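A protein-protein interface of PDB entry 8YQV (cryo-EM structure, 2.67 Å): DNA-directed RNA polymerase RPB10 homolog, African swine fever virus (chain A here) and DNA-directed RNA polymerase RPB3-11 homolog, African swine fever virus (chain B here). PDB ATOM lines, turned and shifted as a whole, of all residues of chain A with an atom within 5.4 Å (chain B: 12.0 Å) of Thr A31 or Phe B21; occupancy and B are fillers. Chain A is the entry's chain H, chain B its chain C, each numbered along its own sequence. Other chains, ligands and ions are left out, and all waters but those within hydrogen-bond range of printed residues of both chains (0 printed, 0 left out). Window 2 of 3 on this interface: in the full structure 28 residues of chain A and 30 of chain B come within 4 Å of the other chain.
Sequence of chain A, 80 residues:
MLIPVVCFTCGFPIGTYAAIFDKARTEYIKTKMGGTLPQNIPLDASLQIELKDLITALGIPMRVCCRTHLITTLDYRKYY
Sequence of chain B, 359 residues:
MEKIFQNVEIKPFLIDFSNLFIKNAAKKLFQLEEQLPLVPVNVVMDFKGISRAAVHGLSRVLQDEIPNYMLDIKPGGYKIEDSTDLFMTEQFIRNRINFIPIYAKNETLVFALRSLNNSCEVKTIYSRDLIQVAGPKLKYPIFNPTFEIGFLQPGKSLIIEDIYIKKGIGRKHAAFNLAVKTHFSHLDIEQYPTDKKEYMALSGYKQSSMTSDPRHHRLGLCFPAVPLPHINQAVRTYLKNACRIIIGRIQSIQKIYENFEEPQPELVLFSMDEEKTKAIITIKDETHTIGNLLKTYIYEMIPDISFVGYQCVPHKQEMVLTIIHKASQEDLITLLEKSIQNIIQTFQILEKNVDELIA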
ATOM      1  N   ALA A  24      18.876 -11.835  16.748  1.00  0.00           N
ATOM      2  CA  ALA A  24      20.269 -11.591  16.404  1.00  0.00           C
ATOM      3  C   ALA A  24      21.049 -12.892  16.342  1.00  0.00           C
ATOM      4  O   ALA A  24      21.724 -13.162  15.343  1.00  0.00           O
ATOM      5  CB  ALA A  24      20.901 -10.637  17.409  1.00  0.00           C
ATOM      6  N   THR A  26      20.148 -15.913  15.714  1.00  0.00           N
ATOM      7  CA  THR A  26      19.824 -16.649  14.502  1.00  0.00           C
ATOM      8  C   THR A  26      20.561 -16.055  13.313  1.00  0.00           C
ATOM      9  O   THR A  26      21.313 -16.754  12.624  1.00  0.00           O
ATOM     10  CB  THR A  26      18.314 -16.641  14.278  1.00  0.00           C
ATOM     11  OG1 THR A  26      17.710 -17.657  15.086  1.00  0.00           O
ATOM     12  CG2 THR A  26      17.992 -16.908  12.835  1.00  0.00           C
ATOM     13  N   GLU A  27      20.444 -14.740  13.129  1.00  0.00           N
ATOM     14  CA  GLU A  27      21.111 -14.111  12.001  1.00  0.00           C
ATOM     15  C   GLU A  27      22.605 -14.353  12.055  1.00  0.00           C
ATOM     16  O   GLU A  27      23.207 -14.735  11.044  1.00  0.00           O
ATOM     17  CB  GLU A  27      20.809 -12.618  11.975  1.00  0.00           C
ATOM     18  CG  GLU A  27      19.383 -12.295  11.594  1.00  0.00           C
ATOM     19  CD  GLU A  27      18.965 -12.960  10.300  1.00  0.00           C
ATOM     20  OE1 GLU A  27      17.799 -13.394  10.202  1.00  0.00           O
ATOM     21  OE2 GLU A  27      19.796 -13.030   9.371  1.00  0.00           O
ATOM     22  N   TYR A  28      23.199 -14.223  13.242  1.00  0.00           N
ATOM     23  CA  TYR A  28      24.633 -14.423  13.365  1.00  0.00           C
ATOM     24  C   TYR A  28      25.023 -15.811  12.890  1.00  0.00           C
ATOM     25  O   TYR A  28      25.974 -15.964  12.117  1.00  0.00           O
ATOM     26  CB  TYR A  28      25.062 -14.198  14.811  1.00  0.00           C
ATOM     27  CG  TYR A  28      26.554 -14.120  15.004  1.00  0.00           C
ATOM     28  CD1 TYR A  28      27.286 -13.089  14.449  1.00  0.00           C
ATOM     29  CD2 TYR A  28      27.227 -15.066  15.757  1.00  0.00           C
ATOM     30  CE1 TYR A  28      28.641 -13.008  14.623  1.00  0.00           C
ATOM     31  CE2 TYR A  28      28.580 -14.991  15.933  1.00  0.00           C
ATOM     32  CZ  TYR A  28      29.284 -13.960  15.366  1.00  0.00           C
ATOM     33  OH  TYR A  28      30.645 -13.880  15.543  1.00  0.00           O
ATOM     34  N   ILE A  29      24.256 -16.828  13.281  1.00  0.00           N
ATOM     35  CA  ILE A  29      24.616 -18.172  12.861  1.00  0.00           C
ATOM     36  C   ILE A  29      24.469 -18.315  11.353  1.00  0.00           C
ATOM     37  O   ILE A  29      25.315 -18.937  10.702  1.00  0.00           O
ATOM     38  CB  ILE A  29      23.792 -19.211  13.635  1.00  0.00           C
ATOM     39  CG1 ILE A  29      24.234 -19.224  15.100  1.00  0.00           C
ATOM     40  CG2 ILE A  29      23.951 -20.581  13.020  1.00  0.00           C
ATOM     41  CD1 ILE A  29      23.351 -20.032  15.996  1.00  0.00           C
ATOM     42  N   LYS A  30      23.439 -17.705  10.760  1.00  0.00           N
ATOM     43  CA  LYS A  30      23.338 -17.771   9.309  1.00  0.00           C
ATOM     44  C   LYS A  30      24.515 -17.112   8.615  1.00  0.00           C
ATOM     45  O   LYS A  30      24.813 -17.469   7.472  1.00  0.00           O
ATOM     46  CB  LYS A  30      22.043 -17.134   8.809  1.00  0.00           C
ATOM     47  CG  LYS A  30      20.897 -18.107   8.635  1.00  0.00           C
ATOM     48  CD  LYS A  30      19.550 -17.407   8.649  1.00  0.00           C
ATOM     49  CE  LYS A  30      18.496 -18.245   9.353  1.00  0.00           C
ATOM     50  NZ  LYS A  30      17.307 -17.443   9.735  1.00  0.00           N
ATOM     51  N   THR A  31      25.195 -16.174   9.269  1.00  0.00           N
ATOM     52  CA  THR A  31      26.396 -15.614   8.671  1.00  0.00           C
ATOM     53  C   THR A  31      27.548 -16.605   8.714  1.00  0.00           C
ATOM     54  O   THR A  31      28.321 -16.696   7.755  1.00  0.00           O
ATOM     55  CB  THR A  31      26.769 -14.307   9.373  1.00  0.00           C
ATOM     56  OG1 THR A  31      25.977 -13.241   8.840  1.00  0.00           O
ATOM     57  CG2 THR A  31      28.233 -13.974   9.177  1.00  0.00           C
ATOM     58  N   LYS A  32      27.650 -17.388   9.785  1.00  0.00           N
ATOM     59  CA  LYS A  32      28.780 -18.286   9.957  1.00  0.00           C
ATOM     60  C   LYS A  32      28.616 -19.612   9.231  1.00  0.00           C
ATOM     61  O   LYS A  32      29.594 -20.353   9.104  1.00  0.00           O
ATOM     62  CB  LYS A  32      29.014 -18.553  11.445  1.00  0.00           C
ATOM     63  CG  LYS A  32      29.099 -17.300  12.290  1.00  0.00           C
ATOM     64  CD  LYS A  32      30.096 -16.319  11.711  1.00  0.00           C
ATOM     65  CE  LYS A  32      31.161 -15.975  12.724  1.00  0.00           C
ATOM     66  NZ  LYS A  32      31.925 -17.186  13.105  1.00  0.00           N
ATOM     67  N   MET A  33      27.416 -19.928   8.756  1.00  0.00           N
ATOM     68  CA  MET A  33      27.202 -21.183   8.047  1.00  0.00           C
ATOM     69  C   MET A  33      27.302 -21.018   6.537  1.00  0.00           C
ATOM     70  O   MET A  33      27.965 -21.818   5.870  1.00  0.00           O
ATOM     71  CB  MET A  33      25.841 -21.768   8.418  1.00  0.00           C
ATOM     72  CG  MET A  33      25.675 -22.004   9.899  1.00  0.00           C
ATOM     73  SD  MET A  33      27.171 -22.617  10.689  1.00  0.00           S
ATOM     74  CE  MET A  33      26.501 -23.974  11.639  1.00  0.00           C
ATOM     75  N   GLY A  34      26.653 -19.998   5.985  1.00  0.00           N
ATOM     76  CA  GLY A  34      26.732 -19.749   4.562  1.00  0.00           C
ATOM     77  C   GLY A  34      25.582 -20.328   3.764  1.00  0.00           C
ATOM     78  O   GLY A  34      25.800 -20.927   2.706  1.00  0.00           O
ATOM     79  N   LEU A  54      28.429 -10.996  20.955  1.00  0.00           N
ATOM     80  CA  LEU A  54      27.037 -10.609  20.763  1.00  0.00           C
ATOM     81  C   LEU A  54      26.370 -10.276  22.092  1.00  0.00           C
ATOM     82  O   LEU A  54      25.708  -9.237  22.229  1.00  0.00           O
ATOM     83  CB  LEU A  54      26.303 -11.744  20.055  1.00  0.00           C
ATOM     84  CG  LEU A  54      25.023 -11.499  19.270  1.00  0.00           C
ATOM     85  CD1 LEU A  54      25.328 -10.719  18.020  1.00  0.00           C
ATOM     86  CD2 LEU A  54      24.420 -12.829  18.924  1.00  0.00           C
ATOM     87  N   ILE B  15      23.021  -0.674  25.371  1.00  0.00           N
ATOM     88  CA  ILE B  15      23.028  -1.547  24.203  1.00  0.00           C
ATOM     89  C   ILE B  15      24.015  -0.992  23.188  1.00  0.00           C
ATOM     90  O   ILE B  15      24.117   0.225  23.007  1.00  0.00           O
ATOM     91  CB  ILE B  15      21.622  -1.666  23.596  1.00  0.00           C
ATOM     92  CG1 ILE B  15      20.646  -2.261  24.605  1.00  0.00           C
ATOM     93  CG2 ILE B  15      21.643  -2.530  22.359  1.00  0.00           C
ATOM     94  CD1 ILE B  15      19.219  -2.275  24.127  1.00  0.00           C
ATOM     95  N   ASP B  16      24.756  -1.882  22.537  1.00  0.00           N
ATOM     96  CA  ASP B  16      25.714  -1.491  21.510  1.00  0.00           C
ATOM     97  C   ASP B  16      25.055  -1.639  20.146  1.00  0.00           C
ATOM     98  O   ASP B  16      24.867  -2.755  19.656  1.00  0.00           O
ATOM     99  CB  ASP B  16      26.976  -2.342  21.600  1.00  0.00           C
ATOM    100  CG  ASP B  16      28.127  -1.750  20.828  1.00  0.00           C
ATOM    101  OD1 ASP B  16      27.991  -0.612  20.343  1.00  0.00           O
ATOM    102  OD2 ASP B  16      29.167  -2.422  20.701  1.00  0.00           O
ATOM    103  N   PHE B  17      24.713  -0.517  19.529  1.00  0.00           N
ATOM    104  CA  PHE B  17      24.134  -0.523  18.198  1.00  0.00           C
ATOM    105  C   PHE B  17      25.191  -0.432  17.110  1.00  0.00           C
ATOM    106  O   PHE B  17      24.846  -0.355  15.928  1.00  0.00           O
ATOM    107  CB  PHE B  17      23.117   0.608  18.064  1.00  0.00           C
ATOM    108  CG  PHE B  17      21.897   0.415  18.909  1.00  0.00           C
ATOM    109  CD1 PHE B  17      20.942  -0.518  18.561  1.00  0.00           C
ATOM    110  CD2 PHE B  17      21.716   1.151  20.058  1.00  0.00           C
ATOM    111  CE1 PHE B  17      19.826  -0.707  19.338  1.00  0.00           C
ATOM    112  CE2 PHE B  17      20.598   0.967  20.839  1.00  0.00           C
ATOM    113  CZ  PHE B  17      19.654   0.038  20.478  1.00  0.00           C
ATOM    114  N   SER B  18      26.469  -0.425  17.488  1.00  0.00           N
ATOM    115  CA  SER B  18      27.548  -0.628  16.535  1.00  0.00           C
ATOM    116  C   SER B  18      27.622  -2.070  16.060  1.00  0.00           C
ATOM    117  O   SER B  18      28.254  -2.340  15.035  1.00  0.00           O
ATOM    118  CB  SER B  18      28.881  -0.224  17.160  1.00  0.00           C
ATOM    119  OG  SER B  18      28.860   1.133  17.553  1.00  0.00           O
ATOM    120  N   ASN B  19      27.007  -2.994  16.790  1.00  0.00           N
ATOM    121  CA  ASN B  19      26.863  -4.369  16.337  1.00  0.00           C
ATOM    122  C   ASN B  19      25.709  -4.437  15.349  1.00  0.00           C
ATOM    123  O   ASN B  19      24.577  -4.087  15.688  1.00  0.00           O
ATOM    124  CB  ASN B  19      26.621  -5.295  17.526  1.00  0.00           C
ATOM    125  CG  ASN B  19      26.746  -6.756  17.162  1.00  0.00           C
ATOM    126  OD1 ASN B  19      26.030  -7.255  16.302  1.00  0.00           O
ATOM    127  ND2 ASN B  19      27.661  -7.451  17.817  1.00  0.00           N
ATOM    128  N   LEU B  20      25.995  -4.880  14.126  1.00  0.00           N
ATOM    129  CA  LEU B  20      24.976  -4.884  13.085  1.00  0.00           C
ATOM    130  C   LEU B  20      23.837  -5.845  13.402  1.00  0.00           C
ATOM    131  O   LEU B  20      22.675  -5.524  13.145  1.00  0.00           O
ATOM    132  CB  LEU B  20      25.604  -5.236  11.739  1.00  0.00           C
ATOM    133  CG  LEU B  20      25.766  -4.064  10.773  1.00  0.00           C
ATOM    134  CD1 LEU B  20      24.408  -3.578  10.311  1.00  0.00           C
ATOM    135  CD2 LEU B  20      26.547  -2.936  11.423  1.00  0.00           C
ATOM    136  N   PHE B  21      24.146  -7.020  13.946  1.00  0.00           N
ATOM    137  CA  PHE B  21      23.102  -8.000  14.225  1.00  0.00           C
ATOM    138  C   PHE B  21      22.141  -7.499  15.296  1.00  0.00           C
ATOM    139  O   PHE B  21      20.918  -7.590  15.132  1.00  0.00           O
ATOM    140  CB  PHE B  21      23.740  -9.321  14.638  1.00  0.00           C
ATOM    141  CG  PHE B  21      24.657  -9.889  13.601  1.00  0.00           C
ATOM    142  CD1 PHE B  21      24.169 -10.702  12.597  1.00  0.00           C
ATOM    143  CD2 PHE B  21      26.003  -9.588  13.613  1.00  0.00           C
ATOM    144  CE1 PHE B  21      25.009 -11.213  11.639  1.00  0.00           C
ATOM    145  CE2 PHE B  21      26.845 -10.094  12.655  1.00  0.00           C
ATOM    146  CZ  PHE B  21      26.347 -10.908  11.668  1.00  0.00           C
ATOM    147  N   ILE B  22      22.677  -6.960  16.392  1.00  0.00           N
ATOM    148  CA  ILE B  22      21.839  -6.401  17.446  1.00  0.00           C
ATOM    149  C   ILE B  22      21.025  -5.237  16.908  1.00  0.00           C
ATOM    150  O   ILE B  22      19.835  -5.099  17.209  1.00  0.00           O
ATOM    151  CB  ILE B  22      22.703  -5.981  18.648  1.00  0.00           C
ATOM    152  CG1 ILE B  22      23.398  -7.195  19.250  1.00  0.00           C
ATOM    153  CG2 ILE B  22      21.871  -5.284  19.698  1.00  0.00           C
ATOM    154  CD1 ILE B  22      22.456  -8.247  19.723  1.00  0.00           C
ATOM    155  N   LYS B  23      21.656  -4.384  16.101  1.00  0.00           N
ATOM    156  CA  LYS B  23      20.960  -3.244  15.517  1.00  0.00           C
ATOM    157  C   LYS B  23      19.772  -3.693  14.681  1.00  0.00           C
ATOM    158  O   LYS B  23      18.659  -3.184  14.842  1.00  0.00           O
ATOM    159  CB  LYS B  23      21.935  -2.429  14.673  1.00  0.00           C
ATOM    160  CG  LYS B  23      21.313  -1.260  13.945  1.00  0.00           C
ATOM    161  CD  LYS B  23      22.351  -0.541  13.109  1.00  0.00           C
ATOM    162  CE  LYS B  23      21.721   0.536  12.255  1.00  0.00           C
ATOM    163  NZ  LYS B  23      21.167   1.636  13.081  1.00  0.00           N
ATOM    164  N   ASN B  24      19.987  -4.658  13.787  1.00  0.00           N
ATOM    165  CA  ASN B  24      18.914  -5.094  12.899  1.00  0.00           C
ATOM    166  C   ASN B  24      17.803  -5.795  13.671  1.00  0.00           C
ATOM    167  O   ASN B  24      16.615  -5.570  13.397  1.00  0.00           O
ATOM    168  CB  ASN B  24      19.473  -6.006  11.811  1.00  0.00           C
ATOM    169  CG  ASN B  24      20.457  -5.297  10.907  1.00  0.00           C
ATOM    170  OD1 ASN B  24      20.354  -4.093  10.681  1.00  0.00           O
ATOM    171  ND2 ASN B  24      21.409  -6.045  10.369  1.00  0.00           N
ATOM    172  N   ALA B  25      18.163  -6.645  14.635  1.00  0.00           N
ATOM    173  CA  ALA B  25      17.145  -7.323  15.429  1.00  0.00           C
ATOM    174  C   ALA B  25      16.307  -6.330  16.219  1.00  0.00           C
ATOM    175  O   ALA B  25      15.076  -6.434  16.245  1.00  0.00           O
ATOM    176  CB  ALA B  25      17.794  -8.337  16.365  1.00  0.00           C
ATOM    177  N   ALA B  26      16.947  -5.349  16.859  1.00  0.00           N
ATOM    178  CA  ALA B  26      16.184  -4.336  17.574  1.00  0.00           C
ATOM    179  C   ALA B  26      15.302  -3.537  16.630  1.00  0.00           C
ATOM    180  O   ALA B  26      14.140  -3.270  16.949  1.00  0.00           O
ATOM    181  CB  ALA B  26      17.127  -3.408  18.335  1.00  0.00           C
ATOM    182  N   LYS B  27      15.828  -3.173  15.459  1.00  0.00           N
ATOM    183  CA  LYS B  27      15.074  -2.366  14.509  1.00  0.00           C
ATOM    184  C   LYS B  27      13.811  -3.080  14.056  1.00  0.00           C
ATOM    185  O   LYS B  27      12.732  -2.483  14.018  1.00  0.00           O
ATOM    186  CB  LYS B  27      15.955  -2.028  13.309  1.00  0.00           C
ATOM    187  CG  LYS B  27      15.210  -1.465  12.117  1.00  0.00           C
ATOM    188  CD  LYS B  27      14.705  -0.066  12.383  1.00  0.00           C
ATOM    189  CE  LYS B  27      13.992   0.507  11.174  1.00  0.00           C
ATOM    190  NZ  LYS B  27      14.914   0.682  10.023  1.00  0.00           N
ATOM    191  N   LYS B  28      13.919  -4.360  13.711  1.00  0.00           N
ATOM    192  CA  LYS B  28      12.782  -5.057  13.129  1.00  0.00           C
ATOM    193  C   LYS B  28      12.004  -5.891  14.144  1.00  0.00           C
ATOM    194  O   LYS B  28      11.070  -6.602  13.763  1.00  0.00           O
ATOM    195  CB  LYS B  28      13.233  -5.897  11.936  1.00  0.00           C
ATOM    196  CG  LYS B  28      13.622  -7.315  12.225  1.00  0.00           C
ATOM    197  CD  LYS B  28      14.070  -8.002  10.943  1.00  0.00           C
ATOM    198  CE  LYS B  28      15.017  -7.128  10.135  1.00  0.00           C
ATOM    199  NZ  LYS B  28      15.025  -7.503   8.695  1.00  0.00           N
ATOM    200  N   LEU B  29      12.345  -5.801  15.427  1.00  0.00           N
ATOM    201  CA  LEU B  29      11.469  -6.286  16.484  1.00  0.00           C
ATOM    202  C   LEU B  29      10.716  -5.166  17.184  1.00  0.00           C
ATOM    203  O   LEU B  29       9.502  -5.263  17.365  1.00  0.00           O
ATOM    204  CB  LEU B  29      12.267  -7.085  17.522  1.00  0.00           C
ATOM    205  CG  LEU B  29      12.306  -8.604  17.396  1.00  0.00           C
ATOM    206  CD1 LEU B  29      13.300  -9.184  18.372  1.00  0.00           C
ATOM    207  CD2 LEU B  29      10.933  -9.179  17.651  1.00  0.00           C
ATOM    208  N   PHE B  30      11.405  -4.097  17.587  1.00  0.00           N
ATOM    209  CA  PHE B  30      10.781  -3.060  18.387  1.00  0.00           C
ATOM    210  C   PHE B  30      10.965  -1.656  17.834  1.00  0.00           C
ATOM    211  O   PHE B  30      10.614  -0.694  18.524  1.00  0.00           O
ATOM    212  CB  PHE B  30      11.321  -3.098  19.825  1.00  0.00           C
ATOM    213  CG  PHE B  30      11.277  -4.458  20.458  1.00  0.00           C
ATOM    214  CD1 PHE B  30      10.074  -5.028  20.823  1.00  0.00           C
ATOM    215  CD2 PHE B  30      12.440  -5.160  20.694  1.00  0.00           C
ATOM    216  CE1 PHE B  30      10.034  -6.269  21.402  1.00  0.00           C
ATOM    217  CE2 PHE B  30      12.400  -6.403  21.272  1.00  0.00           C
ATOM    218  CZ  PHE B  30      11.197  -6.956  21.628  1.00  0.00           C
ATOM    219  N   GLN B  31      11.470  -1.508  16.607  1.00  0.00           N
ATOM    220  CA  GLN B  31      11.795  -0.200  16.028  1.00  0.00           C
ATOM    221  C   GLN B  31      12.673   0.607  16.977  1.00  0.00           C
ATOM    222  O   GLN B  31      12.458   1.798  17.205  1.00  0.00           O
ATOM    223  CB  GLN B  31      10.535   0.580  15.640  1.00  0.00           C
ATOM    224  CG  GLN B  31       9.289  -0.269  15.470  1.00  0.00           C
ATOM    225  CD  GLN B  31       9.371  -1.177  14.267  1.00  0.00           C
ATOM    226  OE1 GLN B  31       9.963  -0.824  13.247  1.00  0.00           O
ATOM    227  NE2 GLN B  31       8.783  -2.363  14.382  1.00  0.00           N
ATOM    228  N   LEU B  32      13.683  -0.057  17.520  1.00  0.00           N
ATOM    229  CA  LEU B  32      14.521   0.480  18.584  1.00  0.00           C
ATOM    230  C   LEU B  32      15.860   0.889  17.983  1.00  0.00           C
ATOM    231  O   LEU B  32      16.674   0.040  17.615  1.00  0.00           O
ATOM    232  CB  LEU B  32      14.688  -0.560  19.686  1.00  0.00           C
ATOM    233  CG  LEU B  32      15.330  -0.163  21.009  1.00  0.00           C
ATOM    234  CD1 LEU B  32      14.397   0.717  21.803  1.00  0.00           C
ATOM    235  CD2 LEU B  32      15.685  -1.408  21.790  1.00  0.00           C
ATOM    236  N   GLU B  33      16.079   2.196  17.872  1.00  0.00           N
ATOM    237  CA  GLU B  33      17.363   2.744  17.467  1.00  0.00           C
ATOM    238  C   GLU B  33      18.047   3.500  18.591  1.00  0.00           C
ATOM    239  O   GLU B  33      19.200   3.913  18.434  1.00  0.00           O
ATOM    240  CB  GLU B  33      17.196   3.672  16.258  1.00  0.00           C
ATOM    241  CG  GLU B  33      16.792   2.973  14.982  1.00  0.00           C
ATOM    242  CD  GLU B  33      15.298   2.975  14.773  1.00  0.00           C
ATOM    243  OE1 GLU B  33      14.716   4.072  14.635  1.00  0.00           O
ATOM    244  OE2 GLU B  33      14.701   1.882  14.757  1.00  0.00           O
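OD1 of Asn B19 sits at hydrogen-bond distance from N of Phe B21 (3.0 Å).
N of Ile B22 is in hydrogen-bond range of OD1 of Asn B19 (3.4 Å).
Ala A24 touches Phe B21 (CB to O, 3.8 Å).
CB of Ala A24 touches CD1 of Ile B22, 3.7 Å away.
N of Ala A24 touches CB of Ala B25 (3.7 Å).
Glu A27 touches Phe B21.
CD1 of Tyr A28 touches CE2 of Phe B21, at 3.5 Å.
Thr A31 touches Phe B21 (OG1 to CE1, 3.6 Å).
Leu A54 touches Asn B19 (CD1 to OD1, 3.9 Å).
Phe B21 touches Leu A54.
Thr A31 touches just one residue of chain B: Phe B21 (3.6 Å).
Printed residues of chain A within 4 Å of Phe B21: Ala A24 (3.8 Å), Glu A27 (3.9 Å), Tyr A28 (3.5 Å), Thr A31 (3.6 Å) and Leu A54 (3.99 Å).
Ala A24 touches just these residues of chain B: Phe B21, Ile B22 and Ala B25.
Of chain B, only Phe B21 (3.9 Å) comes within 4 Å of Glu A27.
Tyr A28 touches just one residue of chain B: Phe B21 (3.5 Å).
No residue of chain B comes within 4 Å of Gly A34.
Of the printed residues of chain B, Leu A54 touches Asn B19 (3.9 Å) and Phe B21 (3.99 Å).
Of the printed residues of chain A, Ala B25 touches Ala A24.
Of the printed residues of chain A, Ile B22 touches Ala A24 (3.7 Å).
Of the printed residues of chain A, Asn B19 touches Leu A54.
The nearest residue of chain B that does not touch Thr A31 is Leu B20 (8.5 Å).
The nearest printed residue of chain A that does not touch Phe B21 is Ile A29 (5.9 Å).
The nearest printed residue of chain A that does not touch Asn B19 is Ala A24 (6.2 Å).
Of the 11 printed residues of chain A, 5 touch a printed residue of chain B.
Hydrophobic or aromatic side chains of chain A that line the printed part of chain B: Ala A24, Tyr A28 and Leu A54.
Hydrophobic or aromatic side chains of chain B that line the printed part of chain A: Phe B21, Ile B22 and Ala B25.
Among the printed residues, 8 pairs touch across the chains.
Among the printed residues, no Asp or Glu carboxylate lies within 4 Å of a Lys or Arg side-chain nitrogen of the other chain.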
